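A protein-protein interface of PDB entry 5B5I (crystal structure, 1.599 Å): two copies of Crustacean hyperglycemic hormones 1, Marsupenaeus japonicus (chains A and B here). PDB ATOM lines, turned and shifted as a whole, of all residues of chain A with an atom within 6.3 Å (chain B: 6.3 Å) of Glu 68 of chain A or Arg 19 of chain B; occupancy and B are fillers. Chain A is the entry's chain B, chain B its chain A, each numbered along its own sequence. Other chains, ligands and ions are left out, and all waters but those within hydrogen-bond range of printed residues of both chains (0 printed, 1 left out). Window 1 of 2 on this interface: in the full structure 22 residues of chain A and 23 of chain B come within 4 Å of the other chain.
No position is printed for both chains.
Of the 13 pairs that touch across the chains among the printed residues, none has its exchanged pair printed and touching as well.
The side-chain carboxylate of Asp 13 of chain B is in salt-bridge range of the guanidinium group of Arg 67 of chain A, 2.8 Å away.
The backbone NH (N) of Asp 13 of chain B sits at hydrogen-bond distance from the backbone carbonyl oxygen (O) of Leu 62 of chain A (3.0 Å).
OE2 of Glu 68 of chain A sits close to OD2 of Asp 13 of chain B, 2.7 Å away.
The guanidinium group (NH2) of Arg 19 of chain B is in salt-bridge range of the side-chain carboxylate (OE1) of Glu 68 of chain A, 3.5 Å away.
N of Arg 14 of chain B sits close to NH2 of Arg 67 of chain A, 3.1 Å away.
Printed residues of chain A that touch a printed residue of chain B: His 61, Leu 62, Asn 64, His 66, Arg 67 and Glu 68.
Among the printed residues, 13 pairs touch across the chains.
The side-chain amide oxygen of Asn 64 of chain A is in hydrogen-bond range of the backbone NH of His 66 of chain A, at 2.9 Å.
The backbone NH (N) of Leu 16 of chain B sits at hydrogen-bond distance from the side-chain carboxylate (OD1) of Asp 13 of chain B, at 3.0 Å.
OD1 of Asp 13 of chain B lies close to N of Gln 15 of chain B, 3.2 Å away.
OH of Tyr 45 of chain B lies within hydrogen-bond range of O of Leu 17 of chain B, 2.7 Å away.
Glu 68 of chain A touches just these residues of chain B: Asp 13, Leu 16 and Arg 19.
Arg 19 of chain B touches just one residue of chain A: Glu 68.
Printed residues of chain B within 4 Å of Arg 67 of chain A: Asp 13, Arg 14 and Gln 15.
Of the printed residues of chain B, His 66 of chain A touches Asp 13 (3.5 Å).
Printed residues of chain B within 4 Å of Asn 64 of chain A: Asp 13.
Printed residues of chain A within 4 Å of Leu 16 of chain B: His 61, Leu 62 and Glu 68.
Printed residues of chain B within 4 Å of Leu 62 of chain A: Asp 13 (3.0 Å), Leu 16 (3.9 Å) and Leu 17 (3.7 Å).
The nearest residue of chain A that does not touch Arg 19 of chain B is Ala 69 of chain A (5.2 Å).
His 61 of chain A touches Asp 13 of chain B.
Leu 16 of chain B touches His 61 of chain A.
CG of Leu 16 of chain B touches CD2 of Leu 62 of chain A, at 3.9 Å.
Leu 62 of chain A touches Leu 17 of chain B.
Asn 64 of chain A touches Asp 13 of chain B (O to CB, 3.5 Å).
O of His 66 of chain A touches OD2 of Asp 13 of chain B (3.5 Å).
Arg 67 of chain A touches Gln 15 of chain B (NE to CB, 3.5 Å).
Leu 16 of chain B touches Glu 68 of chain A (CB to OE1, 3.8 Å).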
ATOM      1  N   HIS A  61      -0.635  -3.703  -1.612  1.00  0.00           N
ATOM      2  CA  HIS A  61      -0.270  -4.322  -0.342  1.00  0.00           C
ATOM      3  C   HIS A  61      -1.174  -5.504   0.002  1.00  0.00           C
ATOM      4  O   HIS A  61      -0.724  -6.453   0.662  1.00  0.00           O
ATOM      5  CB  HIS A  61      -0.302  -3.278   0.774  1.00  0.00           C
ATOM      6  CG  HIS A  61       0.788  -2.257   0.688  1.00  0.00           C
ATOM      7  ND1 HIS A  61       1.009  -1.329   1.682  1.00  0.00           N
ATOM      8  CD2 HIS A  61       1.722  -2.020  -0.262  1.00  0.00           C
ATOM      9  CE1 HIS A  61       2.034  -0.564   1.349  1.00  0.00           C
ATOM     10  NE2 HIS A  61       2.494  -0.971   0.180  1.00  0.00           N
ATOM     11  N   LEU A  62      -2.442  -5.465  -0.420  1.00  0.00           N
ATOM     12  CA  LEU A  62      -3.359  -6.576  -0.173  1.00  0.00           C
ATOM     13  C   LEU A  62      -2.952  -7.811  -0.961  1.00  0.00           C
ATOM     14  O   LEU A  62      -3.134  -8.939  -0.487  1.00  0.00           O
ATOM     15  CB  LEU A  62      -4.792  -6.173  -0.542  1.00  0.00           C
ATOM     16  CG  LEU A  62      -5.521  -5.294   0.457  1.00  0.00           C
ATOM     17  CD1 LEU A  62      -6.851  -4.867  -0.147  1.00  0.00           C
ATOM     18  CD2 LEU A  62      -5.726  -6.049   1.761  1.00  0.00           C
ATOM     19  N   ASN A  64       0.092  -8.671  -1.650  1.00  0.00           N
ATOM     20  CA  ASN A  64       1.443  -9.073  -1.263  1.00  0.00           C
ATOM     21  C   ASN A  64       1.441  -9.635   0.155  1.00  0.00           C
ATOM     22  O   ASN A  64       1.056  -8.938   1.102  1.00  0.00           O
ATOM     23  CB  ASN A  64       2.418  -7.899  -1.365  1.00  0.00           C
ATOM     24  CG  ASN A  64       3.867  -8.310  -1.103  1.00  0.00           C
ATOM     25  OD1 ASN A  64       4.139  -9.399  -0.592  1.00  0.00           O
ATOM     26  ND2 ASN A  64       4.803  -7.427  -1.443  1.00  0.00           N
ATOM     27  N   HIS A  66       3.638  -9.888   2.238  1.00  0.00           N
ATOM     28  CA  HIS A  66       4.473  -9.141   3.173  1.00  0.00           C
ATOM     29  C   HIS A  66       3.630  -8.198   4.025  1.00  0.00           C
ATOM     30  O   HIS A  66       2.988  -7.282   3.503  1.00  0.00           O
ATOM     31  CB  HIS A  66       5.539  -8.357   2.411  1.00  0.00           C
ATOM     32  CG  HIS A  66       6.623  -9.217   1.837  1.00  0.00           C
ATOM     33  ND1 HIS A  66       7.104  -9.049   0.556  1.00  0.00           N
ATOM     34  CD2 HIS A  66       7.324 -10.245   2.373  1.00  0.00           C
ATOM     35  CE1 HIS A  66       8.050  -9.943   0.325  1.00  0.00           C
ATOM     36  NE2 HIS A  66       8.204 -10.679   1.412  1.00  0.00           N
ATOM     37  N   ARG A  67       3.649  -8.421   5.337  1.00  0.00           N
ATOM     38  CA  ARG A  67       2.837  -7.641   6.255  1.00  0.00           C
ATOM     39  C   ARG A  67       3.500  -6.302   6.562  1.00  0.00           C
ATOM     40  O   ARG A  67       4.711  -6.118   6.398  1.00  0.00           O
ATOM     41  CB  ARG A  67       2.585  -8.418   7.551  1.00  0.00           C
ATOM     42  CG  ARG A  67       1.800  -9.711   7.362  1.00  0.00           C
ATOM     43  CD  ARG A  67       0.746  -9.537   6.286  1.00  0.00           C
ATOM     44  NE  ARG A  67      -0.493 -10.245   6.581  1.00  0.00           N
ATOM     45  CZ  ARG A  67      -0.849 -11.403   6.030  1.00  0.00           C
ATOM     46  NH1 ARG A  67      -0.055 -11.998   5.147  1.00  0.00           N
ATOM     47  NH2 ARG A  67      -2.003 -11.966   6.368  1.00  0.00           N
ATOM     48  N   GLU A  68       2.680  -5.359   7.026  1.00  0.00           N
ATOM     49  CA  GLU A  68       3.106  -3.978   7.204  1.00  0.00           C
ATOM     50  C   GLU A  68       3.628  -3.691   8.603  1.00  0.00           C
ATOM     51  O   GLU A  68       4.532  -2.863   8.758  1.00  0.00           O
ATOM     52  CB  GLU A  68       1.947  -3.021   6.893  1.00  0.00           C
ATOM     53  CG  GLU A  68       1.508  -3.013   5.436  1.00  0.00           C
ATOM     54  CD  GLU A  68       0.808  -4.288   5.031  1.00  0.00           C
ATOM     55  OE1 GLU A  68       0.161  -4.915   5.896  1.00  0.00           O
ATOM     56  OE2 GLU A  68       0.919  -4.666   3.851  1.00  0.00           O
ATOM     57  N   ALA A  69       3.080  -4.345   9.622  1.00  0.00           N
ATOM     58  CA  ALA A  69       3.515  -4.116  10.993  1.00  0.00           C
ATOM     59  C   ALA A  69       4.908  -4.688  11.221  1.00  0.00           C
ATOM     60  O   ALA A  69       5.145  -5.874  10.998  1.00  0.00           O
ATOM     61  CB  ALA A  69       2.522  -4.717  11.972  1.00  0.00           C
ATOM     62  N   ASP B  13      -2.784 -10.537   2.074  1.00  0.00           N
ATOM     63  CA  ASP B  13      -2.496  -9.846   3.326  1.00  0.00           C
ATOM     64  C   ASP B  13      -3.828  -9.633   4.039  1.00  0.00           C
ATOM     65  O   ASP B  13      -4.416  -8.553   3.973  1.00  0.00           O
ATOM     66  CB  ASP B  13      -1.785  -8.555   3.053  1.00  0.00           C
ATOM     67  CG  ASP B  13      -1.350  -7.855   4.320  1.00  0.00           C
ATOM     68  OD1 ASP B  13      -1.887  -8.170   5.404  1.00  0.00           O
ATOM     69  OD2 ASP B  13      -0.468  -6.984   4.226  1.00  0.00           O
ATOM     70  N   ARG B  14      -4.300 -10.672   4.729  1.00  0.00           N
ATOM     71  CA  ARG B  14      -5.567 -10.559   5.446  1.00  0.00           C
ATOM     72  C   ARG B  14      -5.464  -9.641   6.660  1.00  0.00           C
ATOM     73  O   ARG B  14      -6.494  -9.153   7.137  1.00  0.00           O
ATOM     74  CB  ARG B  14      -6.060 -11.946   5.871  1.00  0.00           C
ATOM     75  CG  ARG B  14      -6.551 -12.814   4.725  1.00  0.00           C
ATOM     76  CD  ARG B  14      -7.929 -12.369   4.235  1.00  0.00           C
ATOM     77  NE  ARG B  14      -8.376 -13.132   3.069  1.00  0.00           N
ATOM     78  CZ  ARG B  14      -9.581 -13.022   2.514  1.00  0.00           C
ATOM     79  NH1 ARG B  14     -10.476 -12.186   3.019  1.00  0.00           N
ATOM     80  NH2 ARG B  14      -9.900 -13.755   1.455  1.00  0.00           N
ATOM     81  N   GLN B  15      -4.251  -9.395   7.164  1.00  0.00           N
ATOM     82  CA  GLN B  15      -4.076  -8.461   8.273  1.00  0.00           C
ATOM     83  C   GLN B  15      -4.514  -7.056   7.884  1.00  0.00           C
ATOM     84  O   GLN B  15      -5.262  -6.393   8.617  1.00  0.00           O
ATOM     85  CB  GLN B  15      -2.614  -8.449   8.718  1.00  0.00           C
ATOM     86  CG  GLN B  15      -2.317  -7.445   9.810  1.00  0.00           C
ATOM     87  CD  GLN B  15      -1.882  -8.108  11.088  1.00  0.00           C
ATOM     88  OE1 GLN B  15      -1.552  -9.293  11.100  1.00  0.00           O
ATOM     89  NE2 GLN B  15      -1.891  -7.351  12.182  1.00  0.00           N
ATOM     90  N   LEU B  16      -4.034  -6.577   6.735  1.00  0.00           N
ATOM     91  CA  LEU B  16      -4.421  -5.257   6.243  1.00  0.00           C
ATOM     92  C   LEU B  16      -5.905  -5.200   5.888  1.00  0.00           C
ATOM     93  O   LEU B  16      -6.557  -4.161   6.072  1.00  0.00           O
ATOM     94  CB  LEU B  16      -3.564  -4.900   5.025  1.00  0.00           C
ATOM     95  CG  LEU B  16      -3.940  -3.658   4.219  1.00  0.00           C
ATOM     96  CD1 LEU B  16      -3.849  -2.430   5.080  1.00  0.00           C
ATOM     97  CD2 LEU B  16      -3.023  -3.512   3.007  1.00  0.00           C
ATOM     98  N   LEU B  17      -6.447  -6.285   5.333  1.00  0.00           N
ATOM     99  CA  LEU B  17      -7.872  -6.309   5.040  1.00  0.00           C
ATOM    100  C   LEU B  17      -8.676  -6.071   6.310  1.00  0.00           C
ATOM    101  O   LEU B  17      -9.664  -5.334   6.298  1.00  0.00           O
ATOM    102  CB  LEU B  17      -8.259  -7.641   4.393  1.00  0.00           C
ATOM    103  CG  LEU B  17      -9.541  -7.647   3.552  1.00  0.00           C
ATOM    104  CD1 LEU B  17      -9.387  -6.790   2.300  1.00  0.00           C
ATOM    105  CD2 LEU B  17      -9.886  -9.071   3.183  1.00  0.00           C
ATOM    106  N   ARG B  18      -8.239  -6.654   7.428  1.00  0.00           N
ATOM    107  CA  ARG B  18      -8.953  -6.458   8.686  1.00  0.00           C
ATOM    108  C   ARG B  18      -8.784  -5.037   9.217  1.00  0.00           C
ATOM    109  O   ARG B  18      -9.755  -4.431   9.690  1.00  0.00           O
ATOM    110  CB  ARG B  18      -8.484  -7.481   9.716  1.00  0.00           C
ATOM    111  CG  ARG B  18      -8.786  -8.898   9.311  1.00  0.00           C
ATOM    112  CD  ARG B  18      -9.017  -9.767  10.524  1.00  0.00           C
ATOM    113  NE  ARG B  18      -9.248 -11.155  10.146  1.00  0.00           N
ATOM    114  CZ  ARG B  18      -8.278 -12.026   9.899  1.00  0.00           C
ATOM    115  NH1 ARG B  18      -8.576 -13.271   9.567  1.00  0.00           N
ATOM    116  NH2 ARG B  18      -7.011 -11.645   9.985  1.00  0.00           N
ATOM    117  N   ARG B  19      -7.559  -4.496   9.171  1.00  0.00           N
ATOM    118  CA  ARG B  19      -7.335  -3.101   9.543  1.00  0.00           C
ATOM    119  C   ARG B  19      -8.267  -2.175   8.776  1.00  0.00           C
ATOM    120  O   ARG B  19      -8.863  -1.256   9.347  1.00  0.00           O
ATOM    121  CB  ARG B  19      -5.880  -2.693   9.277  1.00  0.00           C
ATOM    122  CG  ARG B  19      -4.829  -3.519   9.989  1.00  0.00           C
ATOM    123  CD  ARG B  19      -3.655  -2.652  10.461  1.00  0.00           C
ATOM    124  NE  ARG B  19      -2.922  -1.989   9.383  1.00  0.00           N
ATOM    125  CZ  ARG B  19      -2.120  -2.602   8.517  1.00  0.00           C
ATOM    126  NH1 ARG B  19      -1.490  -1.897   7.588  1.00  0.00           N
ATOM    127  NH2 ARG B  19      -1.949  -3.918   8.567  1.00  0.00           N
ATOM    128  N   LEU B  20      -8.372  -2.373   7.460  1.00  0.00           N
ATOM    129  CA  LEU B  20      -9.231  -1.508   6.671  1.00  0.00           C
ATOM    130  C   LEU B  20     -10.684  -1.663   7.086  1.00  0.00           C
ATOM    131  O   LEU B  20     -11.437  -0.683   7.117  1.00  0.00           O
ATOM    132  CB  LEU B  20      -9.057  -1.814   5.186  1.00  0.00           C
ATOM    133  CG  LEU B  20      -7.646  -1.594   4.666  1.00  0.00           C
ATOM    134  CD1 LEU B  20      -7.527  -2.283   3.319  1.00  0.00           C
ATOM    135  CD2 LEU B  20      -7.307  -0.122   4.567  1.00  0.00           C
ATOM    136  N   GLY B  21     -11.092  -2.888   7.423  1.00  0.00           N
ATOM    137  CA  GLY B  21     -12.442  -3.107   7.904  1.00  0.00           C
ATOM    138  C   GLY B  21     -12.763  -2.287   9.135  1.00  0.00           C
ATOM    139  O   GLY B  21     -13.922  -1.910   9.348  1.00  0.00           O
ATOM    140  N   ARG B  22     -11.748  -1.996   9.955  1.00  0.00           N
ATOM    141  CA  ARG B  22     -11.979  -1.207  11.159  1.00  0.00           C
ATOM    142  C   ARG B  22     -12.397   0.223  10.825  1.00  0.00           C
ATOM    143  O   ARG B  22     -13.087   0.858  11.624  1.00  0.00           O
ATOM    144  CB  ARG B  22     -10.731  -1.222  12.043  1.00  0.00           C
ATOM    145  CG  ARG B  22     -10.353  -2.614  12.502  1.00  0.00           C
ATOM    146  CD  ARG B  22      -9.082  -2.627  13.331  1.00  0.00           C
ATOM    147  NE  ARG B  22      -8.804  -3.966  13.841  1.00  0.00           N
ATOM    148  CZ  ARG B  22      -7.751  -4.704  13.501  1.00  0.00           C
ATOM    149  NH1 ARG B  22      -6.844  -4.232  12.662  1.00  0.00           N
ATOM    150  NH2 ARG B  22      -7.598  -5.912  14.020  1.00  0.00           N
ATOM    151  N   VAL B  23     -11.998   0.751   9.664  1.00  0.00           N
ATOM    152  CA  VAL B  23     -12.525   2.047   9.242  1.00  0.00           C
ATOM    153  C   VAL B  23     -14.041   1.981   9.132  1.00  0.00           C
ATOM    154  O   VAL B  23     -14.757   2.871   9.605  1.00  0.00           O
ATOM    155  CB  VAL B  23     -11.880   2.496   7.917  1.00  0.00           C
ATOM    156  CG1 VAL B  23     -12.566   3.742   7.398  1.00  0.00           C
ATOM    157  CG2 VAL B  23     -10.399   2.765   8.131  1.00  0.00           C
ATOM    158  N   CYS B  24     -14.557   0.915   8.516  1.00  0.00           N
ATOM    159  CA  CYS B  24     -15.999   0.777   8.372  1.00  0.00           C
ATOM    160  C   CYS B  24     -16.658   0.633   9.737  1.00  0.00           C
ATOM    161  O   CYS B  24     -17.670   1.279  10.038  1.00  0.00           O
ATOM    162  CB  CYS B  24     -16.321  -0.436   7.493  1.00  0.00           C
ATOM    163  SG  CYS B  24     -15.660  -0.316   5.795  1.00  0.00           S
ATOM    164  N   TYR B  45     -12.404  -2.131  -0.798  1.00  0.00           N
ATOM    165  CA  TYR B  45     -12.631  -0.867  -0.103  1.00  0.00           C
ATOM    166  C   TYR B  45     -12.551   0.335  -1.032  1.00  0.00           C
ATOM    167  O   TYR B  45     -12.584   1.472  -0.556  1.00  0.00           O
ATOM    168  CB  TYR B  45     -11.662  -0.670   1.067  1.00  0.00           C
ATOM    169  CG  TYR B  45     -11.748  -1.753   2.108  1.00  0.00           C
ATOM    170  CD1 TYR B  45     -12.752  -1.738   3.070  1.00  0.00           C
ATOM    171  CD2 TYR B  45     -10.823  -2.785   2.139  1.00  0.00           C
ATOM    172  CE1 TYR B  45     -12.833  -2.740   4.042  1.00  0.00           C
ATOM    173  CE2 TYR B  45     -10.896  -3.785   3.103  1.00  0.00           C
ATOM    174  CZ  TYR B  45     -11.897  -3.755   4.048  1.00  0.00           C
ATOM    175  OH  TYR B  45     -11.958  -4.751   5.000  1.00  0.00           O
